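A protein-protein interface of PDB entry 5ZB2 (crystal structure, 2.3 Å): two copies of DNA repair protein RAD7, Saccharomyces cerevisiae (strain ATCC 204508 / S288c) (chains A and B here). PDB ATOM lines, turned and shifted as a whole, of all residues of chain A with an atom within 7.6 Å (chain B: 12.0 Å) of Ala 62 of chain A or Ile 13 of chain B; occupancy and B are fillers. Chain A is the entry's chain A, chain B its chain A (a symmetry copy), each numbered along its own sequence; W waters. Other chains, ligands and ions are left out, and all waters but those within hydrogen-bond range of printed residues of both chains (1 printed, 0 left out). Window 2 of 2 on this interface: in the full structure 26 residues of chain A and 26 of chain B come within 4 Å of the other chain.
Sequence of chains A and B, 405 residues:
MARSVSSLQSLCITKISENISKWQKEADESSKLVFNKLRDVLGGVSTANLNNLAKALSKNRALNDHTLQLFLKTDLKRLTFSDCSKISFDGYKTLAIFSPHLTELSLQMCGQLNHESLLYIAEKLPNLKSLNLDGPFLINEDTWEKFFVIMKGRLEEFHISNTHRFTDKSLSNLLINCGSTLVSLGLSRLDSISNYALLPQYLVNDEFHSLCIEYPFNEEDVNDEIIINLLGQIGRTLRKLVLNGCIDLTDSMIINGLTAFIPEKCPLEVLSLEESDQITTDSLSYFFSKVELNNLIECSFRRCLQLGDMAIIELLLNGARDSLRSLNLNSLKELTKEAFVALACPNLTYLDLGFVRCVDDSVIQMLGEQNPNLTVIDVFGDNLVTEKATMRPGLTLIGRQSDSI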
ATOM      1  N   LEU A  53       5.167 -13.945  34.021  1.00  0.00           N
ATOM      2  CA  LEU A  53       4.333 -13.195  33.090  1.00  0.00           C
ATOM      3  C   LEU A  53       3.636 -12.042  33.801  1.00  0.00           C
ATOM      4  O   LEU A  53       3.632 -10.907  33.312  1.00  0.00           O
ATOM      5  CB  LEU A  53       3.317 -14.132  32.437  1.00  0.00           C
ATOM      6  CG  LEU A  53       2.275 -13.496  31.512  1.00  0.00           C
ATOM      7  CD1 LEU A  53       2.932 -12.726  30.375  1.00  0.00           C
ATOM      8  CD2 LEU A  53       1.345 -14.567  30.963  1.00  0.00           C
ATOM      9  N   ALA A  54       3.056 -12.313  34.973  1.00  0.00           N
ATOM     10  CA  ALA A  54       2.408 -11.258  35.744  1.00  0.00           C
ATOM     11  C   ALA A  54       3.382 -10.131  36.058  1.00  0.00           C
ATOM     12  O   ALA A  54       3.018  -8.950  35.996  1.00  0.00           O
ATOM     13  CB  ALA A  54       1.823 -11.838  37.033  1.00  0.00           C
ATOM     14  N   ALA A  56       6.072  -9.189  34.315  1.00  0.00           N
ATOM     15  CA  ALA A  56       6.324  -8.410  33.107  1.00  0.00           C
ATOM     16  C   ALA A  56       5.172  -7.452  32.829  1.00  0.00           C
ATOM     17  O   ALA A  56       5.384  -6.266  32.554  1.00  0.00           O
ATOM     18  CB  ALA A  56       6.552  -9.347  31.921  1.00  0.00           C
ATOM     19  N   LEU A  57       3.938  -7.950  32.909  1.00  0.00           N
ATOM     20  CA  LEU A  57       2.779  -7.093  32.686  1.00  0.00           C
ATOM     21  C   LEU A  57       2.714  -5.982  33.730  1.00  0.00           C
ATOM     22  O   LEU A  57       2.490  -4.813  33.395  1.00  0.00           O
ATOM     23  CB  LEU A  57       1.502  -7.935  32.700  1.00  0.00           C
ATOM     24  CG  LEU A  57       1.396  -8.962  31.570  1.00  0.00           C
ATOM     25  CD1 LEU A  57       0.203  -9.879  31.773  1.00  0.00           C
ATOM     26  CD2 LEU A  57       1.304  -8.272  30.208  1.00  0.00           C
ATOM     27  N   SER A  58       2.930  -6.327  35.002  1.00  0.00           N
ATOM     28  CA  SER A  58       2.862  -5.325  36.063  1.00  0.00           C
ATOM     29  C   SER A  58       3.848  -4.191  35.812  1.00  0.00           C
ATOM     30  O   SER A  58       3.482  -3.011  35.867  1.00  0.00           O
ATOM     31  CB  SER A  58       3.131  -5.976  37.423  1.00  0.00           C
ATOM     32  OG  SER A  58       2.093  -6.871  37.784  1.00  0.00           O
ATOM     33  N   LYS A  59       5.111  -4.529  35.531  1.00  0.00           N
ATOM     34  CA  LYS A  59       6.117  -3.499  35.314  1.00  0.00           C
ATOM     35  C   LYS A  59       5.770  -2.595  34.139  1.00  0.00           C
ATOM     36  O   LYS A  59       6.229  -1.449  34.098  1.00  0.00           O
ATOM     37  CB  LYS A  59       7.493  -4.138  35.091  1.00  0.00           C
ATOM     38  CG  LYS A  59       8.213  -4.500  36.377  1.00  0.00           C
ATOM     39  CD  LYS A  59       9.678  -4.823  36.131  1.00  0.00           C
ATOM     40  CE  LYS A  59       9.850  -6.129  35.376  1.00  0.00           C
ATOM     41  NZ  LYS A  59      11.279  -6.547  35.313  1.00  0.00           N
ATOM     42  N   ASN A  60       4.974  -3.080  33.189  1.00  0.00           N
ATOM     43  CA  ASN A  60       4.557  -2.287  32.041  1.00  0.00           C
ATOM     44  C   ASN A  60       3.164  -1.696  32.207  1.00  0.00           C
ATOM     45  O   ASN A  60       2.576  -1.248  31.220  1.00  0.00           O
ATOM     46  CB  ASN A  60       4.610  -3.137  30.769  1.00  0.00           C
ATOM     47  CG  ASN A  60       6.026  -3.492  30.367  1.00  0.00           C
ATOM     48  OD1 ASN A  60       6.715  -2.703  29.724  1.00  0.00           O
ATOM     49  ND2 ASN A  60       6.470  -4.684  30.744  1.00  0.00           N
ATOM     50  N   ARG A  61       2.625  -1.682  33.428  1.00  0.00           N
ATOM     51  CA  ARG A  61       1.276  -1.168  33.680  1.00  0.00           C
ATOM     52  C   ARG A  61       0.268  -1.801  32.725  1.00  0.00           C
ATOM     53  O   ARG A  61      -0.698  -1.166  32.293  1.00  0.00           O
ATOM     54  CB  ARG A  61       1.239   0.358  33.570  1.00  0.00           C
ATOM     55  CG  ARG A  61       2.101   1.076  34.595  1.00  0.00           C
ATOM     56  CD  ARG A  61       2.146   2.581  34.352  1.00  0.00           C
ATOM     57  NE  ARG A  61       0.864   3.246  34.603  1.00  0.00           N
ATOM     58  CZ  ARG A  61      -0.016   3.594  33.665  1.00  0.00           C
ATOM     59  NH1 ARG A  61       0.215   3.349  32.382  1.00  0.00           N
ATOM     60  NH2 ARG A  61      -1.144   4.198  34.015  1.00  0.00           N
ATOM     61  N   ALA A  62       0.494  -3.073  32.397  1.00  0.00           N
ATOM     62  CA  ALA A  62      -0.302  -3.778  31.403  1.00  0.00           C
ATOM     63  C   ALA A  62      -1.187  -4.856  32.016  1.00  0.00           C
ATOM     64  O   ALA A  62      -1.788  -5.641  31.277  1.00  0.00           O
ATOM     65  CB  ALA A  62       0.609  -4.397  30.340  1.00  0.00           C
ATOM     66  N   LEU A  63      -1.274  -4.924  33.340  1.00  0.00           N
ATOM     67  CA  LEU A  63      -2.179  -5.854  34.000  1.00  0.00           C
ATOM     68  C   LEU A  63      -3.532  -5.176  34.181  1.00  0.00           C
ATOM     69  O   LEU A  63      -3.629  -4.131  34.837  1.00  0.00           O
ATOM     70  CB  LEU A  63      -1.607  -6.307  35.341  1.00  0.00           C
ATOM     71  CG  LEU A  63      -2.297  -7.501  36.004  1.00  0.00           C
ATOM     72  CD1 LEU A  63      -2.197  -8.760  35.148  1.00  0.00           C
ATOM     73  CD2 LEU A  63      -1.708  -7.755  37.383  1.00  0.00           C
ATOM     74  N   ASN A  64      -4.568  -5.757  33.581  1.00  0.00           N
ATOM     75  CA  ASN A  64      -5.906  -5.185  33.624  1.00  0.00           C
ATOM     76  C   ASN A  64      -6.909  -6.310  33.390  1.00  0.00           C
ATOM     77  O   ASN A  64      -6.540  -7.483  33.289  1.00  0.00           O
ATOM     78  CB  ASN A  64      -6.043  -4.050  32.601  1.00  0.00           C
ATOM     79  CG  ASN A  64      -5.758  -4.501  31.178  1.00  0.00           C
ATOM     80  OD1 ASN A  64      -6.176  -5.580  30.758  1.00  0.00           O
ATOM     81  ND2 ASN A  64      -5.036  -3.673  30.430  1.00  0.00           N
ATOM     82  N   ASP A  65      -8.193  -5.946  33.315  1.00  0.00           N
ATOM     83  CA  ASP A  65      -9.232  -6.965  33.167  1.00  0.00           C
ATOM     84  C   ASP A  65      -9.069  -7.747  31.869  1.00  0.00           C
ATOM     85  O   ASP A  65      -9.473  -8.914  31.790  1.00  0.00           O
ATOM     86  CB  ASP A  65     -10.620  -6.329  33.213  1.00  0.00           C
ATOM     87  CG  ASP A  65     -11.017  -5.870  34.607  1.00  0.00           C
ATOM     88  OD1 ASP A  65     -10.264  -6.130  35.573  1.00  0.00           O
ATOM     89  OD2 ASP A  65     -12.101  -5.257  34.736  1.00  0.00           O
ATOM     90  N   HIS A  66      -8.493  -7.118  30.846  1.00  0.00           N
ATOM     91  CA  HIS A  66      -8.306  -7.773  29.556  1.00  0.00           C
ATOM     92  C   HIS A  66      -7.214  -8.835  29.644  1.00  0.00           C
ATOM     93  O   HIS A  66      -7.454 -10.018  29.373  1.00  0.00           O
ATOM     94  CB  HIS A  66      -7.969  -6.711  28.502  1.00  0.00           C
ATOM     95  CG  HIS A  66      -8.050  -7.192  27.087  1.00  0.00           C
ATOM     96  ND1 HIS A  66      -9.207  -7.700  26.536  1.00  0.00           N
ATOM     97  CD2 HIS A  66      -7.122  -7.210  26.099  1.00  0.00           C
ATOM     98  CE1 HIS A  66      -8.984  -8.027  25.274  1.00  0.00           C
ATOM     99  NE2 HIS A  66      -7.727  -7.741  24.985  1.00  0.00           N
ATOM    100  N   THR A  67      -6.006  -8.432  30.045  1.00  0.00           N
ATOM    101  CA  THR A  67      -4.895  -9.370  30.153  1.00  0.00           C
ATOM    102  C   THR A  67      -5.061 -10.337  31.316  1.00  0.00           C
ATOM    103  O   THR A  67      -4.428 -11.400  31.317  1.00  0.00           O
ATOM    104  CB  THR A  67      -3.576  -8.608  30.305  1.00  0.00           C
ATOM    105  OG1 THR A  67      -3.658  -7.718  31.423  1.00  0.00           O
ATOM    106  CG2 THR A  67      -3.279  -7.810  29.053  1.00  0.00           C
ATOM    107  N   LEU A  68      -5.891  -9.993  32.304  1.00  0.00           N
ATOM    108  CA  LEU A  68      -6.158 -10.902  33.413  1.00  0.00           C
ATOM    109  C   LEU A  68      -6.580 -12.281  32.928  1.00  0.00           C
ATOM    110  O   LEU A  68      -6.370 -13.278  33.627  1.00  0.00           O
ATOM    111  CB  LEU A  68      -7.246 -10.312  34.314  1.00  0.00           C
ATOM    112  CG  LEU A  68      -7.761 -11.200  35.450  1.00  0.00           C
ATOM    113  CD1 LEU A  68      -6.648 -11.492  36.448  1.00  0.00           C
ATOM    114  CD2 LEU A  68      -8.949 -10.544  36.136  1.00  0.00           C
ATOM    115  N   LEU A  70      -5.350 -14.177  30.822  1.00  0.00           N
ATOM    116  CA  LEU A  70      -4.222 -15.088  30.658  1.00  0.00           C
ATOM    117  C   LEU A  70      -4.015 -15.977  31.880  1.00  0.00           C
ATOM    118  O   LEU A  70      -3.388 -17.039  31.767  1.00  0.00           O
ATOM    119  CB  LEU A  70      -2.947 -14.281  30.386  1.00  0.00           C
ATOM    120  CG  LEU A  70      -2.995 -13.369  29.156  1.00  0.00           C
ATOM    121  CD1 LEU A  70      -1.922 -12.290  29.222  1.00  0.00           C
ATOM    122  CD2 LEU A  70      -2.848 -14.193  27.886  1.00  0.00           C
ATOM    123  N   PHE A  71      -4.530 -15.575  33.039  1.00  0.00           N
ATOM    124  CA  PHE A  71      -4.260 -16.255  34.298  1.00  0.00           C
ATOM    125  C   PHE A  71      -5.453 -17.049  34.815  1.00  0.00           C
ATOM    126  O   PHE A  71      -5.422 -17.516  35.958  1.00  0.00           O
ATOM    127  CB  PHE A  71      -3.826 -15.232  35.351  1.00  0.00           C
ATOM    128  CG  PHE A  71      -2.662 -14.387  34.932  1.00  0.00           C
ATOM    129  CD1 PHE A  71      -2.857 -13.227  34.201  1.00  0.00           C
ATOM    130  CD2 PHE A  71      -1.369 -14.749  35.269  1.00  0.00           C
ATOM    131  CE1 PHE A  71      -1.786 -12.449  33.814  1.00  0.00           C
ATOM    132  CE2 PHE A  71      -0.295 -13.973  34.883  1.00  0.00           C
ATOM    133  CZ  PHE A  71      -0.503 -12.824  34.157  1.00  0.00           C
ATOM    134  N   ASP A  83       1.179  -5.018  40.420  1.00  0.00           N
ATOM    135  CA  ASP A  83       0.456  -3.755  40.241  1.00  0.00           C
ATOM    136  C   ASP A  83      -0.927  -4.086  39.689  1.00  0.00           C
ATOM    137  O   ASP A  83      -1.068  -4.329  38.488  1.00  0.00           O
ATOM    138  CB  ASP A  83       1.210  -2.812  39.313  1.00  0.00           C
ATOM    139  CG  ASP A  83       0.514  -1.464  39.152  1.00  0.00           C
ATOM    140  OD1 ASP A  83      -0.703  -1.374  39.424  1.00  0.00           O
ATOM    141  OD2 ASP A  83       1.183  -0.493  38.744  1.00  0.00           O
ATOM    142  N   LYS A  86      -5.179  -1.264  37.740  1.00  0.00           N
ATOM    143  CA  LYS A  86      -6.158  -1.214  36.663  1.00  0.00           C
ATOM    144  C   LYS A  86      -7.171  -2.356  36.702  1.00  0.00           C
ATOM    145  O   LYS A  86      -8.076  -2.386  35.861  1.00  0.00           O
ATOM    146  CB  LYS A  86      -5.439  -1.212  35.309  1.00  0.00           C
ATOM    147  CG  LYS A  86      -4.564   0.013  35.088  1.00  0.00           C
ATOM    148  CD  LYS A  86      -3.881  -0.021  33.729  1.00  0.00           C
ATOM    149  CE  LYS A  86      -3.060   1.235  33.486  1.00  0.00           C
ATOM    150  NZ  LYS A  86      -2.459   1.259  32.123  1.00  0.00           N
ATOM    151  N   SER B   6       9.644   2.170  20.565  1.00  0.00           N
ATOM    152  CA  SER B   6       8.925   1.402  21.573  1.00  0.00           C
ATOM    153  C   SER B   6       9.747   0.199  22.018  1.00  0.00           C
ATOM    154  O   SER B   6      10.358  -0.497  21.202  1.00  0.00           O
ATOM    155  CB  SER B   6       7.575   0.939  21.025  1.00  0.00           C
ATOM    156  OG  SER B   6       6.768   2.044  20.653  1.00  0.00           O
ATOM    157  N   SER B   7       9.757  -0.045  23.326  1.00  0.00           N
ATOM    158  CA  SER B   7      10.486  -1.180  23.873  1.00  0.00           C
ATOM    159  C   SER B   7       9.915  -2.491  23.346  1.00  0.00           C
ATOM    160  O   SER B   7       8.737  -2.586  22.991  1.00  0.00           O
ATOM    161  CB  SER B   7      10.418  -1.170  25.399  1.00  0.00           C
ATOM    162  OG  SER B   7       9.094  -1.417  25.841  1.00  0.00           O
ATOM    163  N   LEU B   8      10.765  -3.518  23.308  1.00  0.00           N
ATOM    164  CA  LEU B   8      10.303  -4.835  22.884  1.00  0.00           C
ATOM    165  C   LEU B   8       9.218  -5.372  23.809  1.00  0.00           C
ATOM    166  O   LEU B   8       8.344  -6.127  23.365  1.00  0.00           O
ATOM    167  CB  LEU B   8      11.475  -5.816  22.829  1.00  0.00           C
ATOM    168  CG  LEU B   8      11.120  -7.249  22.422  1.00  0.00           C
ATOM    169  CD1 LEU B   8      10.417  -7.288  21.067  1.00  0.00           C
ATOM    170  CD2 LEU B   8      12.369  -8.112  22.400  1.00  0.00           C
ATOM    171  N   GLN B   9       9.262  -5.010  25.092  1.00  0.00           N
ATOM    172  CA  GLN B   9       8.211  -5.426  26.016  1.00  0.00           C
ATOM    173  C   GLN B   9       6.866  -4.847  25.597  1.00  0.00           C
ATOM    174  O   GLN B   9       5.860  -5.561  25.529  1.00  0.00           O
ATOM    175  CB  GLN B   9       8.563  -4.992  27.440  1.00  0.00           C
ATOM    176  CG  GLN B   9       9.846  -5.594  27.978  1.00  0.00           C
ATOM    177  CD  GLN B   9      10.367  -4.854  29.198  1.00  0.00           C
ATOM    178  OE1 GLN B   9      11.351  -4.116  29.115  1.00  0.00           O
ATOM    179  NE2 GLN B   9       9.712  -5.047  30.334  1.00  0.00           N
ATOM    180  N   SER B  10       6.836  -3.545  25.309  1.00  0.00           N
ATOM    181  CA  SER B  10       5.597  -2.905  24.883  1.00  0.00           C
ATOM    182  C   SER B  10       5.063  -3.537  23.605  1.00  0.00           C
ATOM    183  O   SER B  10       3.850  -3.731  23.460  1.00  0.00           O
ATOM    184  CB  SER B  10       5.828  -1.406  24.683  1.00  0.00           C
ATOM    185  OG  SER B  10       4.652  -0.770  24.225  1.00  0.00           O
ATOM    186  N   LEU B  11       5.955  -3.875  22.668  1.00  0.00           N
ATOM    187  CA  LEU B  11       5.515  -4.444  21.398  1.00  0.00           C
ATOM    188  C   LEU B  11       4.902  -5.825  21.596  1.00  0.00           C
ATOM    189  O   LEU B  11       3.868  -6.142  20.998  1.00  0.00           O
ATOM    190  CB  LEU B  11       6.688  -4.512  20.418  1.00  0.00           C
ATOM    191  CG  LEU B  11       7.328  -3.174  20.042  1.00  0.00           C
ATOM    192  CD1 LEU B  11       8.512  -3.403  19.119  1.00  0.00           C
ATOM    193  CD2 LEU B  11       6.315  -2.237  19.394  1.00  0.00           C
ATOM    194  N   CYS B  12       5.524  -6.659  22.432  1.00  0.00           N
ATOM    195  CA  CYS B  12       4.935  -7.958  22.737  1.00  0.00           C
ATOM    196  C   CYS B  12       3.579  -7.798  23.414  1.00  0.00           C
ATOM    197  O   CYS B  12       2.645  -8.560  23.140  1.00  0.00           O
ATOM    198  CB  CYS B  12       5.881  -8.771  23.619  1.00  0.00           C
ATOM    199  SG  CYS B  12       7.419  -9.288  22.803  1.00  0.00           S
ATOM    200  N   ILE B  13       3.452  -6.807  24.301  1.00  0.00           N
ATOM    201  CA  ILE B  13       2.186  -6.594  24.998  1.00  0.00           C
ATOM    202  C   ILE B  13       1.097  -6.192  24.013  1.00  0.00           C
ATOM    203  O   ILE B  13      -0.048  -6.644  24.116  1.00  0.00           O
ATOM    204  CB  ILE B  13       2.370  -5.553  26.119  1.00  0.00           C
ATOM    205  CG1 ILE B  13       3.205  -6.167  27.251  1.00  0.00           C
ATOM    206  CG2 ILE B  13       1.017  -5.063  26.644  1.00  0.00           C
ATOM    207  CD1 ILE B  13       3.603  -5.196  28.339  1.00  0.00           C
ATOM    208  N   THR B  14       1.432  -5.344  23.038  1.00  0.00           N
ATOM    209  CA  THR B  14       0.451  -4.981  22.020  1.00  0.00           C
ATOM    210  C   THR B  14       0.012  -6.206  21.229  1.00  0.00           C
ATOM    211  O   THR B  14      -1.185  -6.400  20.983  1.00  0.00           O
ATOM    212  CB  THR B  14       1.024  -3.915  21.086  1.00  0.00           C
ATOM    213  OG1 THR B  14       1.267  -2.715  21.827  1.00  0.00           O
ATOM    214  CG2 THR B  14       0.055  -3.603  19.939  1.00  0.00           C
ATOM    215  N   LYS B  15       0.964  -7.052  20.827  1.00  0.00           N
ATOM    216  CA  LYS B  15       0.608  -8.262  20.093  1.00  0.00           C
ATOM    217  C   LYS B  15      -0.293  -9.155  20.934  1.00  0.00           C
ATOM    218  O   LYS B  15      -1.311  -9.663  20.450  1.00  0.00           O
ATOM    219  CB  LYS B  15       1.873  -9.010  19.668  1.00  0.00           C
ATOM    220  CG  LYS B  15       1.619 -10.293  18.870  1.00  0.00           C
ATOM    221  CD  LYS B  15       0.713 -10.073  17.655  1.00  0.00           C
ATOM    222  CE  LYS B  15       1.307  -9.080  16.663  1.00  0.00           C
ATOM    223  NZ  LYS B  15       0.392  -8.824  15.516  1.00  0.00           N
ATOM    224  N   ILE B  16       0.067  -9.353  22.203  1.00  0.00           N
ATOM    225  CA  ILE B  16      -0.745 -10.178  23.094  1.00  0.00           C
ATOM    226  C   ILE B  16      -2.146  -9.596  23.219  1.00  0.00           C
ATOM    227  O   ILE B  16      -3.149 -10.294  23.029  1.00  0.00           O
ATOM    228  CB  ILE B  16      -0.065 -10.307  24.468  1.00  0.00           C
ATOM    229  CG1 ILE B  16       1.250 -11.082  24.332  1.00  0.00           C
ATOM    230  CG2 ILE B  16      -0.993 -10.997  25.465  1.00  0.00           C
ATOM    231  CD1 ILE B  16       2.122 -11.050  25.569  1.00  0.00           C
ATOM    232  N   SER B  17      -2.234  -8.307  23.548  1.00  0.00           N
ATOM    233  CA  SER B  17      -3.534  -7.672  23.717  1.00  0.00           C
ATOM    234  C   SER B  17      -4.383  -7.808  22.457  1.00  0.00           C
ATOM    235  O   SER B  17      -5.586  -8.089  22.537  1.00  0.00           O
ATOM    236  CB  SER B  17      -3.342  -6.201  24.088  1.00  0.00           C
ATOM    237  OG  SER B  17      -4.535  -5.643  24.609  1.00  0.00           O
ATOM    238  N   GLU B  18      -3.774  -7.625  21.282  1.00  0.00           N
ATOM    239  CA  GLU B  18      -4.527  -7.744  20.037  1.00  0.00           C
ATOM    240  C   GLU B  18      -5.083  -9.152  19.861  1.00  0.00           C
ATOM    241  O   GLU B  18      -6.225  -9.325  19.416  1.00  0.00           O
ATOM    242  CB  GLU B  18      -3.646  -7.368  18.844  1.00  0.00           C
ATOM    243  CG  GLU B  18      -3.336  -5.885  18.735  1.00  0.00           C
ATOM    244  CD  GLU B  18      -2.459  -5.563  17.540  1.00  0.00           C
ATOM    245  OE1 GLU B  18      -2.449  -4.391  17.107  1.00  0.00           O
ATOM    246  OE2 GLU B  18      -1.782  -6.484  17.032  1.00  0.00           O
ATOM    247  N   ASN B  19      -4.296 -10.172  20.207  1.00  0.00           N
ATOM    248  CA  ASN B  19      -4.760 -11.542  20.025  1.00  0.00           C
ATOM    249  C   ASN B  19      -5.786 -11.950  21.072  1.00  0.00           C
ATOM    250  O   ASN B  19      -6.609 -12.833  20.807  1.00  0.00           O
ATOM    251  CB  ASN B  19      -3.578 -12.510  20.042  1.00  0.00           C
ATOM    252  CG  ASN B  19      -2.909 -12.626  18.687  1.00  0.00           C
ATOM    253  OD1 ASN B  19      -3.349 -13.396  17.832  1.00  0.00           O
ATOM    254  ND2 ASN B  19      -1.846 -11.856  18.480  1.00  0.00           N
ATOM    255  N   ILE B  20      -5.764 -11.337  22.258  1.00  0.00           N
ATOM    256  CA  ILE B  20      -6.840 -11.582  23.215  1.00  0.00           C
ATOM    257  C   ILE B  20      -8.164 -11.106  22.633  1.00  0.00           C
ATOM    258  O   ILE B  20      -9.173 -11.817  22.690  1.00  0.00           O
ATOM    259  CB  ILE B  20      -6.538 -10.906  24.566  1.00  0.00           C
ATOM    260  CG1 ILE B  20      -5.272 -11.500  25.191  1.00  0.00           C
ATOM    261  CG2 ILE B  20      -7.713 -11.084  25.529  1.00  0.00           C
ATOM    262  CD1 ILE B  20      -4.780 -10.754  26.413  1.00  0.00           C
ATOM    263  N   SER B  21      -8.172  -9.910  22.039  1.00  0.00           N
ATOM    264  CA  SER B  21      -9.403  -9.369  21.468  1.00  0.00           C
ATOM    265  C   SER B  21      -9.975 -10.304  20.413  1.00  0.00           C
ATOM    266  O   SER B  21     -11.177 -10.598  20.412  1.00  0.00           O
ATOM    267  CB  SER B  21      -9.137  -7.987  20.874  1.00  0.00           C
ATOM    268  OG  SER B  21      -8.722  -7.080  21.878  1.00  0.00           O
ATOM    269  N   LYS B  22      -9.131 -10.789  19.502  1.00  0.00           N
ATOM    270  CA  LYS B  22      -9.623 -11.711  18.485  1.00  0.00           C
ATOM    271  C   LYS B  22     -10.074 -13.023  19.112  1.00  0.00           C
ATOM    272  O   LYS B  22     -11.073 -13.612  18.685  1.00  0.00           O
ATOM    273  CB  LYS B  22      -8.550 -11.962  17.426  1.00  0.00           C
ATOM    274  CG  LYS B  22      -8.989 -12.907  16.313  1.00  0.00           C
ATOM    275  CD  LYS B  22     -10.283 -12.440  15.647  1.00  0.00           C
ATOM    276  CE  LYS B  22     -10.841 -13.478  14.696  1.00  0.00           C
ATOM    277  NZ  LYS B  22     -12.220 -13.117  14.269  1.00  0.00           N
HETATM  278  O   HOH W   1      -4.311  -4.181  27.412  1.00  0.00           O
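ND2 of Asn 60 of chain A lies close to NE2 of Gln 9 of chain B (3.3 Å).
A ring nitrogen (NE2) of His 66 of chain A sits at hydrogen-bond distance from the backbone carbonyl oxygen of Ser 17 of chain B, at 3.3 Å.
A ring nitrogen (NE2) of His 66 of chain A sits at hydrogen-bond distance from the side-chain hydroxyl of Ser 21 of chain B, at 3.3 Å.
The backbone carbonyl oxygen (O) of Ala 56 of chain A lies within hydrogen-bond range of the side-chain amide nitrogen (ND2) of Asn 60 of chain A (2.6 Å).
The backbone carbonyl oxygen (O) of Leu 57 of chain A sits at hydrogen-bond distance from the backbone NH (N) of Ala 62 of chain A, at 2.8 Å.
The side-chain hydroxyl (OG1) of Thr 67 of chain A lies within hydrogen-bond range of the backbone carbonyl oxygen (O) of Ala 62 of chain A (2.8 Å).
The backbone NH of His 66 of chain A is in hydrogen-bond range of the side-chain amide oxygen of Asn 64 of chain A (2.8 Å).
N of Thr 67 of chain A sits at hydrogen-bond distance from OD1 of Asn 64 of chain A (2.9 Å).
OG of Ser 21 of chain B sits at hydrogen-bond distance from O of Ser 17 of chain B.
Among the printed residues, pairs that only touch across the chains: Asn 60 of chain A with Ile 13 of chain B, Ala 62 of chain A with Ile 13 of chain B, His 66 of chain A with Ile 20 of chain B and Thr 67 of chain A with Ile 20 of chain B.
No residue of chain B comes within 4 Å of Ala 56 of chain A.
No residue of chain B comes within 4 Å of Leu 57 of chain A.
No residue of chain B comes within 4 Å of Ser 58 of chain A.
No residue of chain B comes within 4 Å of Arg 61 of chain A.
Ala 62 of chain A touches just one residue of chain B: Ile 13.
No residue of chain B comes within 4 Å of Asn 64 of chain A.
Printed residues of chain B within 4 Å of His 66 of chain A: Ser 17, Ile 20 and Ser 21.
Asp 83 of chain A touches none of the printed residues of chain B.
Of the printed residues of chain A, Gln 9 of chain B touches Asn 60 (3.3 Å).
Ile 13 of chain B touches just these residues of chain A: Asn 60 and Ala 62.
Printed residues of chain A within 4 Å of Ser 17 of chain B: His 66.
Of the printed residues of chain A, Ile 20 of chain B touches His 66 and Thr 67.
Of the printed residues of chain A, Ser 21 of chain B touches His 66 (3.3 Å).
The nearest printed residue of chain B that does not touch Ala 62 of chain A is Ser 17 of chain B (7.2 Å).
The nearest printed residue of chain B that does not touch His 66 of chain A is Glu 18 of chain B (5.4 Å).
Among the printed residues, no Asp or Glu carboxylate lies within 4 Å of a Lys or Arg side-chain nitrogen of the other chain.
No position is printed for both chains.
Of the 7 pairs that touch across the chains among the printed residues, none has its exchanged pair printed and touching as well.
Water W1 bridges ND2 of Asn 64 of chain A (3.1 Å) and OG of Ser 17 of chain B (3.2 Å).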
